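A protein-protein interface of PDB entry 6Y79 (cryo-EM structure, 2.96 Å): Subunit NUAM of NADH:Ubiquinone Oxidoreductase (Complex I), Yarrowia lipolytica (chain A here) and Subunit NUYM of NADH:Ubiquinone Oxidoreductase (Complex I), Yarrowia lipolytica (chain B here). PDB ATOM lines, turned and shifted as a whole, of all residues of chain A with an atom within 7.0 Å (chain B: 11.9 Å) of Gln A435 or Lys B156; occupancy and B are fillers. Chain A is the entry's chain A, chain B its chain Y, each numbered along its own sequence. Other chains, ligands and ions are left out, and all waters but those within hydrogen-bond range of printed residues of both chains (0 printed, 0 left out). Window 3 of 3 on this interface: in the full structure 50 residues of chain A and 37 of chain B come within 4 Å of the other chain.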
ATOM      1  N   ILE A 404      11.320  19.851 -20.788  1.00  0.00           N
ATOM      2  CA  ILE A 404      11.143  18.949 -21.929  1.00  0.00           C
ATOM      3  C   ILE A 404      11.725  17.566 -21.645  1.00  0.00           C
ATOM      4  O   ILE A 404      11.204  16.559 -22.148  1.00  0.00           O
ATOM      5  CB  ILE A 404      11.737  19.594 -23.204  1.00  0.00           C
ATOM      6  CG1 ILE A 404      11.278  18.874 -24.468  1.00  0.00           C
ATOM      7  CG2 ILE A 404      13.254  19.643 -23.191  1.00  0.00           C
ATOM      8  CD1 ILE A 404      11.569  19.674 -25.704  1.00  0.00           C
ATOM      9  N   GLU A 405      12.731  17.498 -20.763  1.00  0.00           N
ATOM     10  CA  GLU A 405      13.310  16.243 -20.301  1.00  0.00           C
ATOM     11  C   GLU A 405      12.278  15.367 -19.598  1.00  0.00           C
ATOM     12  O   GLU A 405      12.385  14.135 -19.629  1.00  0.00           O
ATOM     13  CB  GLU A 405      14.484  16.562 -19.371  1.00  0.00           C
ATOM     14  CG  GLU A 405      15.687  17.217 -20.016  1.00  0.00           C
ATOM     15  CD  GLU A 405      16.768  17.562 -19.013  1.00  0.00           C
ATOM     16  OE1 GLU A 405      16.506  17.464 -17.797  1.00  0.00           O
ATOM     17  OE2 GLU A 405      17.879  17.932 -19.443  1.00  0.00           O
ATOM     18  N   ASP A 406      11.252  15.973 -19.004  1.00  0.00           N
ATOM     19  CA  ASP A 406      10.209  15.224 -18.321  1.00  0.00           C
ATOM     20  C   ASP A 406       9.081  14.778 -19.247  1.00  0.00           C
ATOM     21  O   ASP A 406       8.107  14.197 -18.763  1.00  0.00           O
ATOM     22  CB  ASP A 406       9.637  16.061 -17.173  1.00  0.00           C
ATOM     23  CG  ASP A 406      10.639  16.283 -16.057  1.00  0.00           C
ATOM     24  OD1 ASP A 406      11.510  15.411 -15.859  1.00  0.00           O
ATOM     25  OD2 ASP A 406      10.557  17.329 -15.379  1.00  0.00           O
ATOM     26  N   ALA A 407       9.197  15.003 -20.555  1.00  0.00           N
ATOM     27  CA  ALA A 407       8.060  14.834 -21.454  1.00  0.00           C
ATOM     28  C   ALA A 407       7.726  13.363 -21.723  1.00  0.00           C
ATOM     29  O   ALA A 407       8.584  12.481 -21.634  1.00  0.00           O
ATOM     30  CB  ALA A 407       8.337  15.549 -22.772  1.00  0.00           C
ATOM     31  N   ASP A 408       6.454  13.109 -22.060  1.00  0.00           N
ATOM     32  CA  ASP A 408       5.927  11.778 -22.375  1.00  0.00           C
ATOM     33  C   ASP A 408       5.582  11.614 -23.847  1.00  0.00           C
ATOM     34  O   ASP A 408       6.016  10.648 -24.476  1.00  0.00           O
ATOM     35  CB  ASP A 408       4.671  11.493 -21.533  1.00  0.00           C
ATOM     36  CG  ASP A 408       4.197  10.029 -21.598  1.00  0.00           C
ATOM     37  OD1 ASP A 408       4.819   9.174 -22.267  1.00  0.00           O
ATOM     38  OD2 ASP A 408       3.167   9.732 -20.953  1.00  0.00           O
ATOM     39  N   ARG A 429      15.884  14.837 -28.940  1.00  0.00           N
ATOM     40  CA  ARG A 429      16.516  13.553 -29.240  1.00  0.00           C
ATOM     41  C   ARG A 429      17.096  12.916 -27.985  1.00  0.00           C
ATOM     42  O   ARG A 429      17.045  11.693 -27.825  1.00  0.00           O
ATOM     43  CB  ARG A 429      17.609  13.725 -30.299  1.00  0.00           C
ATOM     44  CG  ARG A 429      18.279  12.412 -30.716  1.00  0.00           C
ATOM     45  CD  ARG A 429      19.300  12.593 -31.823  1.00  0.00           C
ATOM     46  NE  ARG A 429      19.994  11.348 -32.147  1.00  0.00           N
ATOM     47  CZ  ARG A 429      19.516  10.413 -32.964  1.00  0.00           C
ATOM     48  NH1 ARG A 429      18.327  10.560 -33.530  1.00  0.00           N
ATOM     49  NH2 ARG A 429      20.219   9.317 -33.205  1.00  0.00           N
ATOM     50  N   LYS A 430      17.571  13.735 -27.046  1.00  0.00           N
ATOM     51  CA  LYS A 430      18.154  13.219 -25.813  1.00  0.00           C
ATOM     52  C   LYS A 430      17.087  12.613 -24.905  1.00  0.00           C
ATOM     53  O   LYS A 430      17.245  11.487 -24.401  1.00  0.00           O
ATOM     54  CB  LYS A 430      18.895  14.364 -25.127  1.00  0.00           C
ATOM     55  CG  LYS A 430      19.661  14.034 -23.872  1.00  0.00           C
ATOM     56  CD  LYS A 430      20.396  15.280 -23.426  1.00  0.00           C
ATOM     57  CE  LYS A 430      19.410  16.357 -23.012  1.00  0.00           C
ATOM     58  NZ  LYS A 430      18.673  16.117 -21.749  1.00  0.00           N
ATOM     59  N   ALA A 431      15.972  13.330 -24.717  1.00  0.00           N
ATOM     60  CA  ALA A 431      14.866  12.799 -23.921  1.00  0.00           C
ATOM     61  C   ALA A 431      14.196  11.614 -24.607  1.00  0.00           C
ATOM     62  O   ALA A 431      13.768  10.665 -23.933  1.00  0.00           O
ATOM     63  CB  ALA A 431      13.842  13.893 -23.634  1.00  0.00           C
ATOM     64  N   TRP A 432      14.116  11.641 -25.938  1.00  0.00           N
ATOM     65  CA  TRP A 432      13.557  10.530 -26.692  1.00  0.00           C
ATOM     66  C   TRP A 432      14.447   9.302 -26.620  1.00  0.00           C
ATOM     67  O   TRP A 432      13.950   8.170 -26.653  1.00  0.00           O
ATOM     68  CB  TRP A 432      13.365  10.957 -28.143  1.00  0.00           C
ATOM     69  CG  TRP A 432      12.782   9.905 -28.987  1.00  0.00           C
ATOM     70  CD1 TRP A 432      11.540   9.367 -28.877  1.00  0.00           C
ATOM     71  CD2 TRP A 432      13.415   9.241 -30.078  1.00  0.00           C
ATOM     72  NE1 TRP A 432      11.354   8.408 -29.836  1.00  0.00           N
ATOM     73  CE2 TRP A 432      12.493   8.310 -30.587  1.00  0.00           C
ATOM     74  CE3 TRP A 432      14.673   9.340 -30.675  1.00  0.00           C
ATOM     75  CZ2 TRP A 432      12.790   7.486 -31.659  1.00  0.00           C
ATOM     76  CZ3 TRP A 432      14.962   8.525 -31.745  1.00  0.00           C
ATOM     77  CH2 TRP A 432      14.021   7.618 -32.233  1.00  0.00           C
ATOM     78  N   LEU A 433      15.758   9.509 -26.518  1.00  0.00           N
ATOM     79  CA  LEU A 433      16.701   8.412 -26.401  1.00  0.00           C
ATOM     80  C   LEU A 433      16.645   7.781 -25.020  1.00  0.00           C
ATOM     81  O   LEU A 433      16.713   6.554 -24.892  1.00  0.00           O
ATOM     82  CB  LEU A 433      18.109   8.925 -26.696  1.00  0.00           C
ATOM     83  CG  LEU A 433      19.219   7.888 -26.712  1.00  0.00           C
ATOM     84  CD1 LEU A 433      18.892   6.895 -27.784  1.00  0.00           C
ATOM     85  CD2 LEU A 433      20.559   8.548 -26.983  1.00  0.00           C
ATOM     86  N   ARG A 434      16.507   8.602 -23.981  1.00  0.00           N
ATOM     87  CA  ARG A 434      16.485   8.048 -22.631  1.00  0.00           C
ATOM     88  C   ARG A 434      15.129   7.465 -22.237  1.00  0.00           C
ATOM     89  O   ARG A 434      15.078   6.597 -21.359  1.00  0.00           O
ATOM     90  CB  ARG A 434      16.892   9.114 -21.614  1.00  0.00           C
ATOM     91  CG  ARG A 434      15.923  10.248 -21.536  1.00  0.00           C
ATOM     92  CD  ARG A 434      16.339  11.292 -20.587  1.00  0.00           C
ATOM     93  NE  ARG A 434      17.591  11.921 -21.012  1.00  0.00           N
ATOM     94  CZ  ARG A 434      18.245  12.781 -20.248  1.00  0.00           C
ATOM     95  NH1 ARG A 434      17.581  13.710 -19.572  1.00  0.00           N
ATOM     96  NH2 ARG A 434      19.544  12.692 -20.131  1.00  0.00           N
ATOM     97  N   GLN A 435      14.030   7.918 -22.848  1.00  0.00           N
ATOM     98  CA  GLN A 435      12.711   7.548 -22.345  1.00  0.00           C
ATOM     99  C   GLN A 435      11.816   6.941 -23.414  1.00  0.00           C
ATOM    100  O   GLN A 435      12.269   6.617 -24.516  1.00  0.00           O
ATOM    101  CB  GLN A 435      11.999   8.765 -21.747  1.00  0.00           C
ATOM    102  CG  GLN A 435      12.566   9.275 -20.439  1.00  0.00           C
ATOM    103  CD  GLN A 435      11.869  10.533 -19.966  1.00  0.00           C
ATOM    104  OE1 GLN A 435      10.953  11.032 -20.622  1.00  0.00           O
ATOM    105  NE2 GLN A 435      12.320  11.074 -18.841  1.00  0.00           N
ATOM    106  N   GLU A 436      10.541   6.777 -23.075  1.00  0.00           N
ATOM    107  CA  GLU A 436       9.502   6.412 -24.030  1.00  0.00           C
ATOM    108  C   GLU A 436       8.786   7.699 -24.420  1.00  0.00           C
ATOM    109  O   GLU A 436       7.891   8.164 -23.710  1.00  0.00           O
ATOM    110  CB  GLU A 436       8.542   5.389 -23.434  1.00  0.00           C
ATOM    111  CG  GLU A 436       7.481   4.903 -24.403  1.00  0.00           C
ATOM    112  CD  GLU A 436       6.582   3.846 -23.799  1.00  0.00           C
ATOM    113  OE1 GLU A 436       6.781   3.502 -22.614  1.00  0.00           O
ATOM    114  OE2 GLU A 436       5.676   3.359 -24.507  1.00  0.00           O
ATOM    115  N   LEU A 437       9.194   8.282 -25.543  1.00  0.00           N
ATOM    116  CA  LEU A 437       8.644   9.535 -26.033  1.00  0.00           C
ATOM    117  C   LEU A 437       7.997   9.307 -27.393  1.00  0.00           C
ATOM    118  O   LEU A 437       8.489   8.515 -28.203  1.00  0.00           O
ATOM    119  CB  LEU A 437       9.734  10.618 -26.124  1.00  0.00           C
ATOM    120  CG  LEU A 437       9.377  12.049 -26.539  1.00  0.00           C
ATOM    121  CD1 LEU A 437       8.445  12.689 -25.546  1.00  0.00           C
ATOM    122  CD2 LEU A 437      10.619  12.903 -26.679  1.00  0.00           C
ATOM    123  N   THR A 449      16.601  14.562 -36.620  1.00  0.00           N
ATOM    124  CA  THR A 449      17.510  13.562 -36.087  1.00  0.00           C
ATOM    125  C   THR A 449      16.725  12.395 -35.498  1.00  0.00           C
ATOM    126  O   THR A 449      17.077  11.230 -35.710  1.00  0.00           O
ATOM    127  CB  THR A 449      18.416  14.192 -35.034  1.00  0.00           C
ATOM    128  OG1 THR A 449      17.617  14.685 -33.953  1.00  0.00           O
ATOM    129  CG2 THR A 449      19.201  15.344 -35.635  1.00  0.00           C
ATOM    130  N   ASP A 451      12.743  10.478 -34.464  1.00  0.00           N
ATOM    131  CA  ASP A 451      11.663   9.855 -35.227  1.00  0.00           C
ATOM    132  C   ASP A 451      10.379  10.645 -35.011  1.00  0.00           C
ATOM    133  O   ASP A 451       9.880  10.728 -33.883  1.00  0.00           O
ATOM    134  CB  ASP A 451      11.479   8.397 -34.802  1.00  0.00           C
ATOM    135  CG  ASP A 451      10.573   7.600 -35.733  1.00  0.00           C
ATOM    136  OD1 ASP A 451      10.070   8.146 -36.738  1.00  0.00           O
ATOM    137  OD2 ASP A 451      10.363   6.401 -35.445  1.00  0.00           O
ATOM    138  N   LYS B 138      24.158  20.037 -13.380  1.00  0.00           N
ATOM    139  CA  LYS B 138      23.139  19.215 -12.750  1.00  0.00           C
ATOM    140  C   LYS B 138      23.657  17.796 -12.599  1.00  0.00           C
ATOM    141  O   LYS B 138      24.184  17.214 -13.552  1.00  0.00           O
ATOM    142  CB  LYS B 138      21.851  19.217 -13.569  1.00  0.00           C
ATOM    143  CG  LYS B 138      20.709  18.478 -12.897  1.00  0.00           C
ATOM    144  CD  LYS B 138      19.460  18.489 -13.747  1.00  0.00           C
ATOM    145  CE  LYS B 138      19.625  17.605 -14.970  1.00  0.00           C
ATOM    146  NZ  LYS B 138      19.784  16.170 -14.616  1.00  0.00           N
ATOM    147  N   ARG B 140      23.554  14.034 -12.691  1.00  0.00           N
ATOM    148  CA  ARG B 140      22.804  12.975 -13.346  1.00  0.00           C
ATOM    149  C   ARG B 140      23.546  11.667 -13.131  1.00  0.00           C
ATOM    150  O   ARG B 140      24.768  11.617 -13.285  1.00  0.00           O
ATOM    151  CB  ARG B 140      22.644  13.269 -14.836  1.00  0.00           C
ATOM    152  CG  ARG B 140      21.813  12.264 -15.580  1.00  0.00           C
ATOM    153  CD  ARG B 140      20.353  12.627 -15.518  1.00  0.00           C
ATOM    154  NE  ARG B 140      19.519  11.611 -16.145  1.00  0.00           N
ATOM    155  CZ  ARG B 140      18.194  11.667 -16.192  1.00  0.00           C
ATOM    156  NH1 ARG B 140      17.508  10.697 -16.778  1.00  0.00           N
ATOM    157  NH2 ARG B 140      17.557  12.694 -15.648  1.00  0.00           N
ATOM    158  N   VAL B 141      22.817  10.617 -12.773  1.00  0.00           N
ATOM    159  CA  VAL B 141      23.437   9.341 -12.443  1.00  0.00           C
ATOM    160  C   VAL B 141      23.834   8.640 -13.729  1.00  0.00           C
ATOM    161  O   VAL B 141      23.017   8.483 -14.643  1.00  0.00           O
ATOM    162  CB  VAL B 141      22.485   8.467 -11.615  1.00  0.00           C
ATOM    163  CG1 VAL B 141      23.118   7.113 -11.331  1.00  0.00           C
ATOM    164  CG2 VAL B 141      22.095   9.179 -10.334  1.00  0.00           C
ATOM    165  N   ASN B 146      24.302   1.312 -18.661  1.00  0.00           N
ATOM    166  CA  ASN B 146      23.292   2.059 -19.407  1.00  0.00           C
ATOM    167  C   ASN B 146      23.452   1.878 -20.911  1.00  0.00           C
ATOM    168  O   ASN B 146      22.470   1.973 -21.657  1.00  0.00           O
ATOM    169  CB  ASN B 146      23.392   3.539 -19.005  1.00  0.00           C
ATOM    170  CG  ASN B 146      22.556   4.481 -19.876  1.00  0.00           C
ATOM    171  OD1 ASN B 146      22.940   4.843 -20.993  1.00  0.00           O
ATOM    172  ND2 ASN B 146      21.427   4.917 -19.340  1.00  0.00           N
ATOM    173  N   ASN B 147      24.675   1.611 -21.372  1.00  0.00           N
ATOM    174  CA  ASN B 147      24.997   1.655 -22.792  1.00  0.00           C
ATOM    175  C   ASN B 147      24.385   0.513 -23.587  1.00  0.00           C
ATOM    176  O   ASN B 147      24.267   0.631 -24.810  1.00  0.00           O
ATOM    177  CB  ASN B 147      26.516   1.639 -22.978  1.00  0.00           C
ATOM    178  CG  ASN B 147      27.186   2.891 -22.444  1.00  0.00           C
ATOM    179  OD1 ASN B 147      26.670   3.996 -22.589  1.00  0.00           O
ATOM    180  ND2 ASN B 147      28.346   2.719 -21.823  1.00  0.00           N
ATOM    181  N   VAL B 149      21.368  -1.595 -22.621  1.00  0.00           N
ATOM    182  CA  VAL B 149      20.154  -2.146 -22.031  1.00  0.00           C
ATOM    183  C   VAL B 149      19.237  -2.681 -23.125  1.00  0.00           C
ATOM    184  O   VAL B 149      19.324  -2.281 -24.292  1.00  0.00           O
ATOM    185  CB  VAL B 149      19.440  -1.093 -21.168  1.00  0.00           C
ATOM    186  CG1 VAL B 149      20.301  -0.730 -19.978  1.00  0.00           C
ATOM    187  CG2 VAL B 149      19.125   0.132 -21.992  1.00  0.00           C
ATOM    188  N   HIS B 150      18.352  -3.602 -22.748  1.00  0.00           N
ATOM    189  CA  HIS B 150      17.647  -4.401 -23.740  1.00  0.00           C
ATOM    190  C   HIS B 150      16.551  -3.606 -24.430  1.00  0.00           C
ATOM    191  O   HIS B 150      15.736  -2.934 -23.784  1.00  0.00           O
ATOM    192  CB  HIS B 150      17.052  -5.653 -23.103  1.00  0.00           C
ATOM    193  CG  HIS B 150      16.332  -6.526 -24.082  1.00  0.00           C
ATOM    194  ND1 HIS B 150      16.977  -7.171 -25.113  1.00  0.00           N
ATOM    195  CD2 HIS B 150      15.025  -6.858 -24.189  1.00  0.00           C
ATOM    196  CE1 HIS B 150      16.098  -7.861 -25.817  1.00  0.00           C
ATOM    197  NE2 HIS B 150      14.905  -7.690 -25.276  1.00  0.00           N
ATOM    198  N   SER B 151      16.533  -3.699 -25.748  1.00  0.00           N
ATOM    199  CA  SER B 151      15.495  -3.095 -26.559  1.00  0.00           C
ATOM    200  C   SER B 151      14.328  -4.066 -26.658  1.00  0.00           C
ATOM    201  O   SER B 151      14.493  -5.190 -27.137  1.00  0.00           O
ATOM    202  CB  SER B 151      16.032  -2.742 -27.938  1.00  0.00           C
ATOM    203  OG  SER B 151      14.993  -2.363 -28.825  1.00  0.00           O
ATOM    204  N   TYR B 152      13.161  -3.657 -26.142  1.00  0.00           N
ATOM    205  CA  TYR B 152      11.962  -4.461 -26.335  1.00  0.00           C
ATOM    206  C   TYR B 152      11.282  -4.124 -27.655  1.00  0.00           C
ATOM    207  O   TYR B 152      10.906  -5.027 -28.406  1.00  0.00           O
ATOM    208  CB  TYR B 152      11.011  -4.257 -25.170  1.00  0.00           C
ATOM    209  CG  TYR B 152      11.480  -4.909 -23.886  1.00  0.00           C
ATOM    210  CD1 TYR B 152      11.401  -6.289 -23.713  1.00  0.00           C
ATOM    211  CD2 TYR B 152      12.006  -4.148 -22.852  1.00  0.00           C
ATOM    212  CE1 TYR B 152      11.839  -6.886 -22.545  1.00  0.00           C
ATOM    213  CE2 TYR B 152      12.443  -4.732 -21.685  1.00  0.00           C
ATOM    214  CZ  TYR B 152      12.359  -6.096 -21.532  1.00  0.00           C
ATOM    215  OH  TYR B 152      12.803  -6.664 -20.357  1.00  0.00           O
ATOM    216  N   GLY B 153      11.128  -2.837 -27.967  1.00  0.00           N
ATOM    217  CA  GLY B 153      10.508  -2.450 -29.225  1.00  0.00           C
ATOM    218  C   GLY B 153      11.534  -2.089 -30.276  1.00  0.00           C
ATOM    219  O   GLY B 153      12.485  -2.843 -30.500  1.00  0.00           O
ATOM    220  N   LYS B 154      11.343  -0.948 -30.931  1.00  0.00           N
ATOM    221  CA  LYS B 154      12.325  -0.451 -31.881  1.00  0.00           C
ATOM    222  C   LYS B 154      13.609  -0.082 -31.149  1.00  0.00           C
ATOM    223  O   LYS B 154      13.572   0.439 -30.030  1.00  0.00           O
ATOM    224  CB  LYS B 154      11.767   0.760 -32.629  1.00  0.00           C
ATOM    225  CG  LYS B 154      12.672   1.330 -33.707  1.00  0.00           C
ATOM    226  CD  LYS B 154      12.923   0.311 -34.796  1.00  0.00           C
ATOM    227  CE  LYS B 154      11.679   0.103 -35.639  1.00  0.00           C
ATOM    228  NZ  LYS B 154      11.919  -0.838 -36.768  1.00  0.00           N
ATOM    229  N   LEU B 155      14.748  -0.406 -31.773  1.00  0.00           N
ATOM    230  CA  LEU B 155      16.054  -0.089 -31.200  1.00  0.00           C
ATOM    231  C   LEU B 155      16.237   1.406 -31.045  1.00  0.00           C
ATOM    232  O   LEU B 155      16.743   1.870 -30.018  1.00  0.00           O
ATOM    233  CB  LEU B 155      17.178  -0.625 -32.083  1.00  0.00           C
ATOM    234  CG  LEU B 155      17.681  -2.048 -31.901  1.00  0.00           C
ATOM    235  CD1 LEU B 155      16.705  -2.993 -32.516  1.00  0.00           C
ATOM    236  CD2 LEU B 155      19.037  -2.202 -32.547  1.00  0.00           C
ATOM    237  N   LYS B 156      15.912   2.156 -32.100  1.00  0.00           N
ATOM    238  CA  LYS B 156      15.854   3.620 -32.151  1.00  0.00           C
ATOM    239  C   LYS B 156      17.216   4.286 -31.900  1.00  0.00           C
ATOM    240  O   LYS B 156      17.306   5.514 -31.831  1.00  0.00           O
ATOM    241  CB  LYS B 156      14.745   4.149 -31.216  1.00  0.00           C
ATOM    242  CG  LYS B 156      15.037   4.521 -29.756  1.00  0.00           C
ATOM    243  CD  LYS B 156      13.718   4.789 -29.041  1.00  0.00           C
ATOM    244  CE  LYS B 156      13.868   4.985 -27.553  1.00  0.00           C
ATOM    245  NZ  LYS B 156      12.584   5.476 -26.977  1.00  0.00           N
ATOM    246  N   HIS B 157      18.289   3.492 -31.874  1.00  0.00           N
ATOM    247  CA  HIS B 157      19.663   3.906 -31.629  1.00  0.00           C
ATOM    248  C   HIS B 157      20.595   2.730 -31.872  1.00  0.00           C
ATOM    249  O   HIS B 157      20.251   1.580 -31.584  1.00  0.00           O
ATOM    250  CB  HIS B 157      19.865   4.409 -30.199  1.00  0.00           C
ATOM    251  CG  HIS B 157      21.222   4.985 -29.961  1.00  0.00           C
ATOM    252  ND1 HIS B 157      21.731   6.011 -30.725  1.00  0.00           N
ATOM    253  CD2 HIS B 157      22.187   4.663 -29.069  1.00  0.00           C
ATOM    254  CE1 HIS B 157      22.948   6.305 -30.306  1.00  0.00           C
ATOM    255  NE2 HIS B 157      23.248   5.501 -29.303  1.00  0.00           N
ATOM    256  N   ILE B 158      21.786   3.034 -32.381  1.00  0.00           N
ATOM    257  CA  ILE B 158      22.876   2.074 -32.509  1.00  0.00           C
ATOM    258  C   ILE B 158      24.095   2.697 -31.845  1.00  0.00           C
ATOM    259  O   ILE B 158      24.633   3.692 -32.343  1.00  0.00           O
ATOM    260  CB  ILE B 158      23.181   1.719 -33.970  1.00  0.00           C
ATOM    261  CG1 ILE B 158      21.975   1.058 -34.632  1.00  0.00           C
ATOM    262  CG2 ILE B 158      24.381   0.796 -34.057  1.00  0.00           C
ATOM    263  CD1 ILE B 158      22.138   0.880 -36.116  1.00  0.00           C
ATOM    264  N   ARG B 159      24.526   2.130 -30.723  1.00  0.00           N
ATOM    265  CA  ARG B 159      25.757   2.576 -30.094  1.00  0.00           C
ATOM    266  C   ARG B 159      26.960   2.148 -30.936  1.00  0.00           C
ATOM    267  O   ARG B 159      26.862   1.307 -31.832  1.00  0.00           O
ATOM    268  CB  ARG B 159      25.872   2.012 -28.675  1.00  0.00           C
ATOM    269  CG  ARG B 159      24.731   2.383 -27.742  1.00  0.00           C
ATOM    270  CD  ARG B 159      25.057   3.605 -26.898  1.00  0.00           C
ATOM    271  NE  ARG B 159      23.982   3.908 -25.955  1.00  0.00           N
ATOM    272  CZ  ARG B 159      23.762   5.107 -25.423  1.00  0.00           C
ATOM    273  NH1 ARG B 159      22.758   5.281 -24.577  1.00  0.00           N
ATOM    274  NH2 ARG B 159      24.538   6.133 -25.741  1.00  0.00           N
ATOM    275  N   THR B 160      28.109   2.738 -30.638  1.00  0.00           N
ATOM    276  CA  THR B 160      29.356   2.397 -31.322  1.00  0.00           C
ATOM    277  C   THR B 160      30.398   1.798 -30.404  1.00  0.00           C
ATOM    278  O   THR B 160      30.878   0.693 -30.673  1.00  0.00           O
ATOM    279  CB  THR B 160      29.987   3.631 -31.945  1.00  0.00           C
ATOM    280  OG1 THR B 160      30.238   4.593 -30.911  1.00  0.00           O
ATOM    281  CG2 THR B 160      29.102   4.230 -32.965  1.00  0.00           C
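O of Ala A407 lies close to OE1 of Gln A435, 3.0 Å away. The backbone carbonyl oxygen (O) of Lys A430 sits close to the guanidinium group (NE) of Arg A434 (3.4 Å). The backbone carbonyl oxygen (O) of Glu A405 is in hydrogen-bond range of the side-chain amide nitrogen (NE2) of Gln A435, 3.2 Å away. The backbone carbonyl oxygen of Leu A437 lies close to the indole nitrogen of Trp A432, at 3.3 Å.
The backbone carbonyl oxygen of Gln A435 is in hydrogen-bond range of the side-chain amino group of Lys B156 (2.7 Å). O of Trp A432 lies within hydrogen-bond range of NZ of Lys B156, 3.0 Å away.
Among the printed residues, pairs that only touch across the chains: Leu A433 with His B157 (3.6 Å) and Arg A434 with Arg B140 (3.997 Å).
Of the 16 printed residues of chain A, 4 touch a printed residue of chain B. Printed residues of chain A that touch a printed residue of chain B: Trp A432, Leu A433, Arg A434 and Gln A435. Hydrophobic or aromatic side chains of chain A that line the printed part of chain B: Trp A432 and Leu A433. Among the printed residues, 4 pairs touch across the chains. Among the printed residues, no Asp or Glu carboxylate lies within 4 Å of a Lys or Arg side-chain nitrogen of the other chain.
No residue of chain B comes within 4 Å of Asp A406. Arg A429 touches none of the printed residues of chain B. No residue of chain B comes within 4 Å of Ala A431. Of chain B, only Lys B156 comes within 4 Å of Trp A432. Of the printed residues of chain B, Arg A434 touches Arg B140 (3.997 Å). Gln A435 touches just one residue of chain B: Lys B156 (2.7 Å). No residue of chain B comes within 4 Å of Glu A436. No residue of chain B comes within 4 Å of Leu A437. Asn B146 touches none of the printed residues of chain A. Of chain A, only Trp A432 (3.0 Å) and Gln A435 (2.7 Å) come within 4 Å of Lys B156. Of the printed residues of chain A, His B157 touches Leu A433 (3.6 Å). The nearest residue of chain B that does not touch Gln A435 is Arg B140 (5.6 Å). The nearest residue of chain A that does not touch Lys B156 is Leu A433 (4.2 Å). The nearest printed residue of chain A that does not touch His B157 is Arg A429 (4.4 Å).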
